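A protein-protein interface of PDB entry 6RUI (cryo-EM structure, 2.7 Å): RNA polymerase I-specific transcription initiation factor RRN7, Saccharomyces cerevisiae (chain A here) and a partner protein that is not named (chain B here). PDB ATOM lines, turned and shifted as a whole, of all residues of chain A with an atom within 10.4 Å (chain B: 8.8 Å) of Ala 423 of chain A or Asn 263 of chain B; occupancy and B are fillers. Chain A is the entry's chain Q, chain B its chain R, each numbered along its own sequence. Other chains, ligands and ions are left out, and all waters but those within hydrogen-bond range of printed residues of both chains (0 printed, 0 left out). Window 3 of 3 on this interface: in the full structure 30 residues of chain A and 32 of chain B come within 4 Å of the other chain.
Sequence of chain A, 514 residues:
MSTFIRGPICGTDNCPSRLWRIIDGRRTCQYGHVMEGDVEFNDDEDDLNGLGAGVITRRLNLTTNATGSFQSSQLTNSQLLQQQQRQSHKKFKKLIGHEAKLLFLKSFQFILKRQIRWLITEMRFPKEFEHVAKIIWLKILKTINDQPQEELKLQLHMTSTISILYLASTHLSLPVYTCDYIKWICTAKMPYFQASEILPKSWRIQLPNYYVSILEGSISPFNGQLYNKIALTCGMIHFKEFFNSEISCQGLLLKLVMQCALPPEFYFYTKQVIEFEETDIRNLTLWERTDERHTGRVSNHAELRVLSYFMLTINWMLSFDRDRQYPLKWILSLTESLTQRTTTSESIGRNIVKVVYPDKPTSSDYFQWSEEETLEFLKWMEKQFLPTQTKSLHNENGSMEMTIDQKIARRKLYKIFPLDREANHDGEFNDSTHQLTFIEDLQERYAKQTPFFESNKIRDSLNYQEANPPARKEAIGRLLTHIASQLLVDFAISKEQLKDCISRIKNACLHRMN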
ATOM      1  N   LYS A 415      -1.681   4.125  -4.849  1.00  0.00           N
ATOM      2  CA  LYS A 415      -0.262   4.005  -5.147  1.00  0.00           C
ATOM      3  C   LYS A 415       0.475   5.303  -4.860  1.00  0.00           C
ATOM      4  O   LYS A 415       1.633   5.281  -4.431  1.00  0.00           O
ATOM      5  CB  LYS A 415      -0.101   3.596  -6.608  1.00  0.00           C
ATOM      6  CG  LYS A 415       1.313   3.485  -7.114  1.00  0.00           C
ATOM      7  CD  LYS A 415       2.041   2.317  -6.497  1.00  0.00           C
ATOM      8  CE  LYS A 415       3.420   2.179  -7.102  1.00  0.00           C
ATOM      9  NZ  LYS A 415       4.253   3.365  -6.774  1.00  0.00           N
ATOM     10  N   ILE A 416      -0.173   6.444  -5.077  1.00  0.00           N
ATOM     11  CA  ILE A 416       0.509   7.712  -4.854  1.00  0.00           C
ATOM     12  C   ILE A 416       0.290   8.229  -3.433  1.00  0.00           C
ATOM     13  O   ILE A 416       1.134   8.955  -2.903  1.00  0.00           O
ATOM     14  CB  ILE A 416       0.103   8.742  -5.930  1.00  0.00           C
ATOM     15  CG1 ILE A 416       1.017   9.956  -5.916  1.00  0.00           C
ATOM     16  CG2 ILE A 416      -1.289   9.226  -5.773  1.00  0.00           C
ATOM     17  CD1 ILE A 416       0.840  10.818  -7.102  1.00  0.00           C
ATOM     18  N   PHE A 417      -0.786   7.818  -2.764  1.00  0.00           N
ATOM     19  CA  PHE A 417      -0.957   8.074  -1.335  1.00  0.00           C
ATOM     20  C   PHE A 417      -0.941   6.736  -0.617  1.00  0.00           C
ATOM     21  O   PHE A 417      -2.000   6.122  -0.429  1.00  0.00           O
ATOM     22  CB  PHE A 417      -2.265   8.805  -1.037  1.00  0.00           C
ATOM     23  CG  PHE A 417      -2.379  10.142  -1.670  1.00  0.00           C
ATOM     24  CD1 PHE A 417      -1.805  11.252  -1.093  1.00  0.00           C
ATOM     25  CD2 PHE A 417      -3.089  10.289  -2.840  1.00  0.00           C
ATOM     26  CE1 PHE A 417      -1.932  12.479  -1.683  1.00  0.00           C
ATOM     27  CE2 PHE A 417      -3.209  11.507  -3.432  1.00  0.00           C
ATOM     28  CZ  PHE A 417      -2.633  12.601  -2.854  1.00  0.00           C
ATOM     29  N   PRO A 418       0.219   6.227  -0.213  1.00  0.00           N
ATOM     30  CA  PRO A 418       0.224   5.053   0.659  1.00  0.00           C
ATOM     31  C   PRO A 418      -0.344   5.401   2.023  1.00  0.00           C
ATOM     32  O   PRO A 418      -0.113   6.489   2.549  1.00  0.00           O
ATOM     33  CB  PRO A 418       1.703   4.674   0.733  1.00  0.00           C
ATOM     34  CG  PRO A 418       2.426   5.915   0.386  1.00  0.00           C
ATOM     35  CD  PRO A 418       1.579   6.624  -0.600  1.00  0.00           C
ATOM     36  N   LEU A 419      -1.127   4.467   2.571  1.00  0.00           N
ATOM     37  CA  LEU A 419      -1.927   4.747   3.759  1.00  0.00           C
ATOM     38  C   LEU A 419      -1.062   4.916   4.993  1.00  0.00           C
ATOM     39  O   LEU A 419      -1.379   5.731   5.864  1.00  0.00           O
ATOM     40  CB  LEU A 419      -2.958   3.633   3.961  1.00  0.00           C
ATOM     41  CG  LEU A 419      -4.049   3.669   5.041  1.00  0.00           C
ATOM     42  CD1 LEU A 419      -3.608   3.038   6.356  1.00  0.00           C
ATOM     43  CD2 LEU A 419      -4.520   5.100   5.282  1.00  0.00           C
ATOM     44  N   ASP A 420       0.039   4.187   5.073  1.00  0.00           N
ATOM     45  CA  ASP A 420       0.989   4.379   6.154  1.00  0.00           C
ATOM     46  C   ASP A 420       1.819   5.629   5.877  1.00  0.00           C
ATOM     47  O   ASP A 420       1.540   6.401   4.956  1.00  0.00           O
ATOM     48  CB  ASP A 420       1.848   3.130   6.318  1.00  0.00           C
ATOM     49  CG  ASP A 420       2.541   2.721   5.031  1.00  0.00           C
ATOM     50  OD1 ASP A 420       2.255   3.306   3.968  1.00  0.00           O
ATOM     51  OD2 ASP A 420       3.391   1.812   5.087  1.00  0.00           O
ATOM     52  N   ARG A 421       2.856   5.849   6.672  1.00  0.00           N
ATOM     53  CA  ARG A 421       3.843   6.831   6.269  1.00  0.00           C
ATOM     54  C   ARG A 421       4.566   6.299   5.038  1.00  0.00           C
ATOM     55  O   ARG A 421       4.707   5.087   4.852  1.00  0.00           O
ATOM     56  CB  ARG A 421       4.812   7.134   7.415  1.00  0.00           C
ATOM     57  CG  ARG A 421       5.688   8.361   7.181  1.00  0.00           C
ATOM     58  CD  ARG A 421       6.500   8.750   8.403  1.00  0.00           C
ATOM     59  NE  ARG A 421       7.348   9.904   8.121  1.00  0.00           N
ATOM     60  CZ  ARG A 421       8.117  10.507   9.022  1.00  0.00           C
ATOM     61  NH1 ARG A 421       8.860  11.548   8.675  1.00  0.00           N
ATOM     62  NH2 ARG A 421       8.139  10.074  10.274  1.00  0.00           N
ATOM     63  N   GLU A 422       4.955   7.222   4.159  1.00  0.00           N
ATOM     64  CA  GLU A 422       5.564   6.853   2.886  1.00  0.00           C
ATOM     65  C   GLU A 422       6.900   6.140   3.070  1.00  0.00           C
ATOM     66  O   GLU A 422       7.272   5.304   2.237  1.00  0.00           O
ATOM     67  CB  GLU A 422       5.695   8.112   2.034  1.00  0.00           C
ATOM     68  CG  GLU A 422       6.411   9.238   2.742  1.00  0.00           C
ATOM     69  CD  GLU A 422       6.327  10.534   1.979  1.00  0.00           C
ATOM     70  OE1 GLU A 422       5.652  10.561   0.929  1.00  0.00           O
ATOM     71  OE2 GLU A 422       6.946  11.524   2.421  1.00  0.00           O
ATOM     72  N   ALA A 423       7.609   6.431   4.159  1.00  0.00           N
ATOM     73  CA  ALA A 423       8.768   5.666   4.595  1.00  0.00           C
ATOM     74  C   ALA A 423       8.972   5.935   6.076  1.00  0.00           C
ATOM     75  O   ALA A 423       8.580   6.987   6.585  1.00  0.00           O
ATOM     76  CB  ALA A 423      10.030   6.028   3.804  1.00  0.00           C
ATOM     77  N   ASN A 424       9.606   4.967   6.749  1.00  0.00           N
ATOM     78  CA  ASN A 424       9.945   5.022   8.179  1.00  0.00           C
ATOM     79  C   ASN A 424       8.698   5.189   9.051  1.00  0.00           C
ATOM     80  O   ASN A 424       8.479   6.222   9.688  1.00  0.00           O
ATOM     81  CB  ASN A 424      10.978   6.118   8.482  1.00  0.00           C
ATOM     82  CG  ASN A 424      12.347   5.805   7.918  1.00  0.00           C
ATOM     83  OD1 ASN A 424      12.807   4.663   7.966  1.00  0.00           O
ATOM     84  ND2 ASN A 424      13.014   6.824   7.387  1.00  0.00           N
ATOM     85  N   HIS A 425       7.868   4.148   9.049  1.00  0.00           N
ATOM     86  CA  HIS A 425       6.730   4.083   9.954  1.00  0.00           C
ATOM     87  C   HIS A 425       7.188   3.680  11.359  1.00  0.00           C
ATOM     88  O   HIS A 425       8.323   3.244  11.573  1.00  0.00           O
ATOM     89  CB  HIS A 425       5.681   3.101   9.429  1.00  0.00           C
ATOM     90  CG  HIS A 425       6.177   1.695   9.301  1.00  0.00           C
ATOM     91  ND1 HIS A 425       6.131   0.791  10.340  1.00  0.00           N
ATOM     92  CD2 HIS A 425       6.733   1.038   8.256  1.00  0.00           C
ATOM     93  CE1 HIS A 425       6.637  -0.361   9.940  1.00  0.00           C
ATOM     94  NE2 HIS A 425       7.008  -0.238   8.678  1.00  0.00           N
ATOM     95  N   ASP A 426       6.278   3.832  12.321  1.00  0.00           N
ATOM     96  CA  ASP A 426       6.574   3.637  13.740  1.00  0.00           C
ATOM     97  C   ASP A 426       6.125   2.275  14.253  1.00  0.00           C
ATOM     98  O   ASP A 426       5.671   2.151  15.393  1.00  0.00           O
ATOM     99  CB  ASP A 426       5.947   4.760  14.569  1.00  0.00           C
ATOM    100  CG  ASP A 426       4.422   4.859  14.410  1.00  0.00           C
ATOM    101  OD1 ASP A 426       3.828   4.147  13.570  1.00  0.00           O
ATOM    102  OD2 ASP A 426       3.812   5.665  15.149  1.00  0.00           O
ATOM    103  N   GLY A 427       6.237   1.234  13.438  1.00  0.00           N
ATOM    104  CA  GLY A 427       5.756  -0.072  13.837  1.00  0.00           C
ATOM    105  C   GLY A 427       6.773  -0.932  14.556  1.00  0.00           C
ATOM    106  O   GLY A 427       6.503  -1.418  15.659  1.00  0.00           O
ATOM    107  N   TYR B 233      -0.749  15.288   5.714  1.00  0.00           N
ATOM    108  CA  TYR B 233      -0.677  14.165   4.790  1.00  0.00           C
ATOM    109  C   TYR B 233      -1.477  12.983   5.309  1.00  0.00           C
ATOM    110  O   TYR B 233      -2.184  12.321   4.544  1.00  0.00           O
ATOM    111  CB  TYR B 233       0.770  13.746   4.568  1.00  0.00           C
ATOM    112  CG  TYR B 233       0.902  12.580   3.623  1.00  0.00           C
ATOM    113  CD1 TYR B 233       0.765  12.757   2.261  1.00  0.00           C
ATOM    114  CD2 TYR B 233       1.149  11.304   4.096  1.00  0.00           C
ATOM    115  CE1 TYR B 233       0.880  11.701   1.398  1.00  0.00           C
ATOM    116  CE2 TYR B 233       1.255  10.246   3.239  1.00  0.00           C
ATOM    117  CZ  TYR B 233       1.125  10.454   1.895  1.00  0.00           C
ATOM    118  OH  TYR B 233       1.239   9.397   1.040  1.00  0.00           O
ATOM    119  N   LYS B 234      -1.361  12.697   6.604  1.00  0.00           N
ATOM    120  CA  LYS B 234      -1.977  11.500   7.151  1.00  0.00           C
ATOM    121  C   LYS B 234      -3.487  11.620   7.170  1.00  0.00           C
ATOM    122  O   LYS B 234      -4.190  10.632   6.955  1.00  0.00           O
ATOM    123  CB  LYS B 234      -1.452  11.231   8.554  1.00  0.00           C
ATOM    124  CG  LYS B 234      -0.003  10.859   8.614  1.00  0.00           C
ATOM    125  CD  LYS B 234       0.414  10.581  10.038  1.00  0.00           C
ATOM    126  CE  LYS B 234       1.909  10.390  10.136  1.00  0.00           C
ATOM    127  NZ  LYS B 234       2.341   9.169   9.415  1.00  0.00           N
ATOM    128  N   GLU B 256       0.291  19.481  -0.407  1.00  0.00           N
ATOM    129  CA  GLU B 256       0.858  18.606   0.602  1.00  0.00           C
ATOM    130  C   GLU B 256       1.893  17.659   0.029  1.00  0.00           C
ATOM    131  O   GLU B 256       2.836  17.309   0.732  1.00  0.00           O
ATOM    132  CB  GLU B 256      -0.242  17.812   1.273  1.00  0.00           C
ATOM    133  CG  GLU B 256      -1.228  18.675   1.977  1.00  0.00           C
ATOM    134  CD  GLU B 256      -2.333  17.865   2.572  1.00  0.00           C
ATOM    135  OE1 GLU B 256      -2.316  16.630   2.388  1.00  0.00           O
ATOM    136  OE2 GLU B 256      -3.231  18.454   3.200  1.00  0.00           O
ATOM    137  N   ILE B 257       1.750  17.227  -1.222  1.00  0.00           N
ATOM    138  CA  ILE B 257       2.764  16.332  -1.762  1.00  0.00           C
ATOM    139  C   ILE B 257       4.003  17.118  -2.139  1.00  0.00           C
ATOM    140  O   ILE B 257       5.129  16.682  -1.887  1.00  0.00           O
ATOM    141  CB  ILE B 257       2.236  15.535  -2.966  1.00  0.00           C
ATOM    142  CG1 ILE B 257       0.982  14.763  -2.629  1.00  0.00           C
ATOM    143  CG2 ILE B 257       3.240  14.486  -3.384  1.00  0.00           C
ATOM    144  CD1 ILE B 257       0.379  14.146  -3.863  1.00  0.00           C
ATOM    145  N   LEU B 258       3.821  18.290  -2.737  1.00  0.00           N
ATOM    146  CA  LEU B 258       4.968  19.080  -3.155  1.00  0.00           C
ATOM    147  C   LEU B 258       5.701  19.641  -1.947  1.00  0.00           C
ATOM    148  O   LEU B 258       6.931  19.562  -1.864  1.00  0.00           O
ATOM    149  CB  LEU B 258       4.517  20.192  -4.099  1.00  0.00           C
ATOM    150  CG  LEU B 258       5.550  20.998  -4.894  1.00  0.00           C
ATOM    151  CD1 LEU B 258       4.955  21.374  -6.235  1.00  0.00           C
ATOM    152  CD2 LEU B 258       6.013  22.265  -4.174  1.00  0.00           C
ATOM    153  N   ASN B 260       6.149  18.437   0.948  1.00  0.00           N
ATOM    154  CA  ASN B 260       6.502  17.413   1.921  1.00  0.00           C
ATOM    155  C   ASN B 260       7.958  17.047   1.696  1.00  0.00           C
ATOM    156  O   ASN B 260       8.743  16.959   2.645  1.00  0.00           O
ATOM    157  CB  ASN B 260       5.606  16.186   1.775  1.00  0.00           C
ATOM    158  CG  ASN B 260       5.510  15.379   3.043  1.00  0.00           C
ATOM    159  OD1 ASN B 260       6.125  15.716   4.049  1.00  0.00           O
ATOM    160  ND2 ASN B 260       4.719  14.315   3.008  1.00  0.00           N
ATOM    161  N   LEU B 261       8.296  16.798   0.429  1.00  0.00           N
ATOM    162  CA  LEU B 261       9.653  16.676  -0.104  1.00  0.00           C
ATOM    163  C   LEU B 261      10.443  15.496   0.449  1.00  0.00           C
ATOM    164  O   LEU B 261      11.663  15.443   0.267  1.00  0.00           O
ATOM    165  CB  LEU B 261      10.464  17.961   0.116  1.00  0.00           C
ATOM    166  CG  LEU B 261      10.084  19.222  -0.653  1.00  0.00           C
ATOM    167  CD1 LEU B 261      10.948  20.354  -0.165  1.00  0.00           C
ATOM    168  CD2 LEU B 261      10.266  19.025  -2.146  1.00  0.00           C
ATOM    169  N   SER B 262       9.807  14.533   1.110  1.00  0.00           N
ATOM    170  CA  SER B 262      10.578  13.435   1.683  1.00  0.00           C
ATOM    171  C   SER B 262      10.668  12.249   0.726  1.00  0.00           C
ATOM    172  O   SER B 262      11.754  11.898   0.254  1.00  0.00           O
ATOM    173  CB  SER B 262       9.953  12.997   3.012  1.00  0.00           C
ATOM    174  OG  SER B 262      10.640  11.881   3.555  1.00  0.00           O
ATOM    175  N   ASN B 263       9.529  11.648   0.419  1.00  0.00           N
ATOM    176  CA  ASN B 263       9.399  10.552  -0.530  1.00  0.00           C
ATOM    177  C   ASN B 263       8.330  10.916  -1.536  1.00  0.00           C
ATOM    178  O   ASN B 263       7.432  10.144  -1.877  1.00  0.00           O
ATOM    179  CB  ASN B 263       9.079   9.264   0.211  1.00  0.00           C
ATOM    180  CG  ASN B 263      10.143   8.905   1.214  1.00  0.00           C
ATOM    181  OD1 ASN B 263       9.931   9.014   2.419  1.00  0.00           O
ATOM    182  ND2 ASN B 263      11.299   8.477   0.723  1.00  0.00           N
ATOM    183  N   SER B 264       8.435  12.142  -2.015  1.00  0.00           N
ATOM    184  CA  SER B 264       7.307  12.856  -2.571  1.00  0.00           C
ATOM    185  C   SER B 264       7.179  12.609  -4.064  1.00  0.00           C
ATOM    186  O   SER B 264       8.169  12.413  -4.774  1.00  0.00           O
ATOM    187  CB  SER B 264       7.467  14.350  -2.288  1.00  0.00           C
ATOM    188  OG  SER B 264       6.419  15.099  -2.857  1.00  0.00           O
ATOM    189  N   SER B 265       5.934  12.612  -4.531  1.00  0.00           N
ATOM    190  CA  SER B 265       5.632  12.676  -5.950  1.00  0.00           C
ATOM    191  C   SER B 265       5.644  14.104  -6.463  1.00  0.00           C
ATOM    192  O   SER B 265       5.398  14.324  -7.654  1.00  0.00           O
ATOM    193  CB  SER B 265       4.272  12.041  -6.218  1.00  0.00           C
ATOM    194  OG  SER B 265       4.274  10.684  -5.821  1.00  0.00           O
ATOM    195  N   SER B 266       5.891  15.066  -5.567  1.00  0.00           N
ATOM    196  CA  SER B 266       5.984  16.506  -5.816  1.00  0.00           C
ATOM    197  C   SER B 266       4.692  17.085  -6.378  1.00  0.00           C
ATOM    198  O   SER B 266       4.700  18.159  -6.981  1.00  0.00           O
ATOM    199  CB  SER B 266       7.175  16.849  -6.724  1.00  0.00           C
ATOM    200  OG  SER B 266       7.281  18.245  -6.931  1.00  0.00           O
ATOM    201  N   GLY B 267       3.571  16.386  -6.206  1.00  0.00           N
ATOM    202  CA  GLY B 267       2.292  16.868  -6.650  1.00  0.00           C
ATOM    203  C   GLY B 267       2.036  16.762  -8.130  1.00  0.00           C
ATOM    204  O   GLY B 267       0.888  16.911  -8.554  1.00  0.00           O
ATOM    205  N   ASP B 269       2.682  14.133 -10.306  1.00  0.00           N
ATOM    206  CA  ASP B 269       2.069  12.875 -10.691  1.00  0.00           C
ATOM    207  C   ASP B 269       0.635  12.768 -10.217  1.00  0.00           C
ATOM    208  O   ASP B 269      -0.120  11.949 -10.747  1.00  0.00           O
ATOM    209  CB  ASP B 269       2.852  11.691 -10.136  1.00  0.00           C
ATOM    210  CG  ASP B 269       4.171  11.498 -10.823  1.00  0.00           C
ATOM    211  OD1 ASP B 269       4.295  11.924 -11.990  1.00  0.00           O
ATOM    212  OD2 ASP B 269       5.076  10.898 -10.207  1.00  0.00           O
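OE2 of Glu 422 of chain A lies within hydrogen-bond range of N of Asn 263 of chain B, at 3.3 Å.
The side-chain amide oxygen of Asn 263 of chain B is in hydrogen-bond range of the side-chain hydroxyl of Ser 262 of chain B.
Ile 416 of chain A touches Tyr 233 of chain B (O to OH, 3.97 Å). CG1 of Ile 416 of chain A touches OG of Ser 265 of chain B (3.3 Å). Asp 269 of chain B touches Ile 416 of chain A. OH of Tyr 233 of chain B touches CA of Phe 417 of chain A (3.5 Å). CD1 of Ile 257 of chain B touches CZ of Phe 417 of chain A, at 3.5 Å. OH of Tyr 233 of chain B touches CD of Pro 418 of chain A (3.2 Å). Arg 421 of chain A touches Lys 234 of chain B. OE2 of Glu 422 of chain A touches ND2 of Asn 260 of chain B, 3.6 Å away. Ser 262 of chain B touches Glu 422 of chain A. CB of Ala 423 of chain A touches OD1 of Asn 263 of chain B (3.3 Å).
Of chain B, only Asn 263 comes within 4 Å of Ala 423 of chain A. No residue of chain B comes within 4 Å of Asn 424 of chain A. Of the printed residues of chain A, Asn 263 of chain B touches Glu 422 and Ala 423. Of the printed residues of chain A, Ser 265 of chain B touches Ile 416 (3.3 Å). Of the printed residues of chain A, Asp 269 of chain B touches Ile 416. The nearest residue of chain B that does not touch Ala 423 of chain A is Ser 262 of chain B (5.9 Å). The nearest residue of chain A that does not touch Asn 263 of chain B is Asn 424 of chain A (5.9 Å).
Of the 14 printed residues of chain B, 8 touch a printed residue of chain A. Printed residues of chain B that touch a printed residue of chain A: Tyr 233, Lys 234, Ile 257, Asn 260, Ser 262, Asn 263, Ser 265 and Asp 269. Of the 13 printed residues of chain A, 6 touch a printed residue of chain B. Hydrophobic or aromatic side chains of chain A within 4 Å of the printed part of chain B: Ile 416, Phe 417, Pro 418 and Ala 423.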
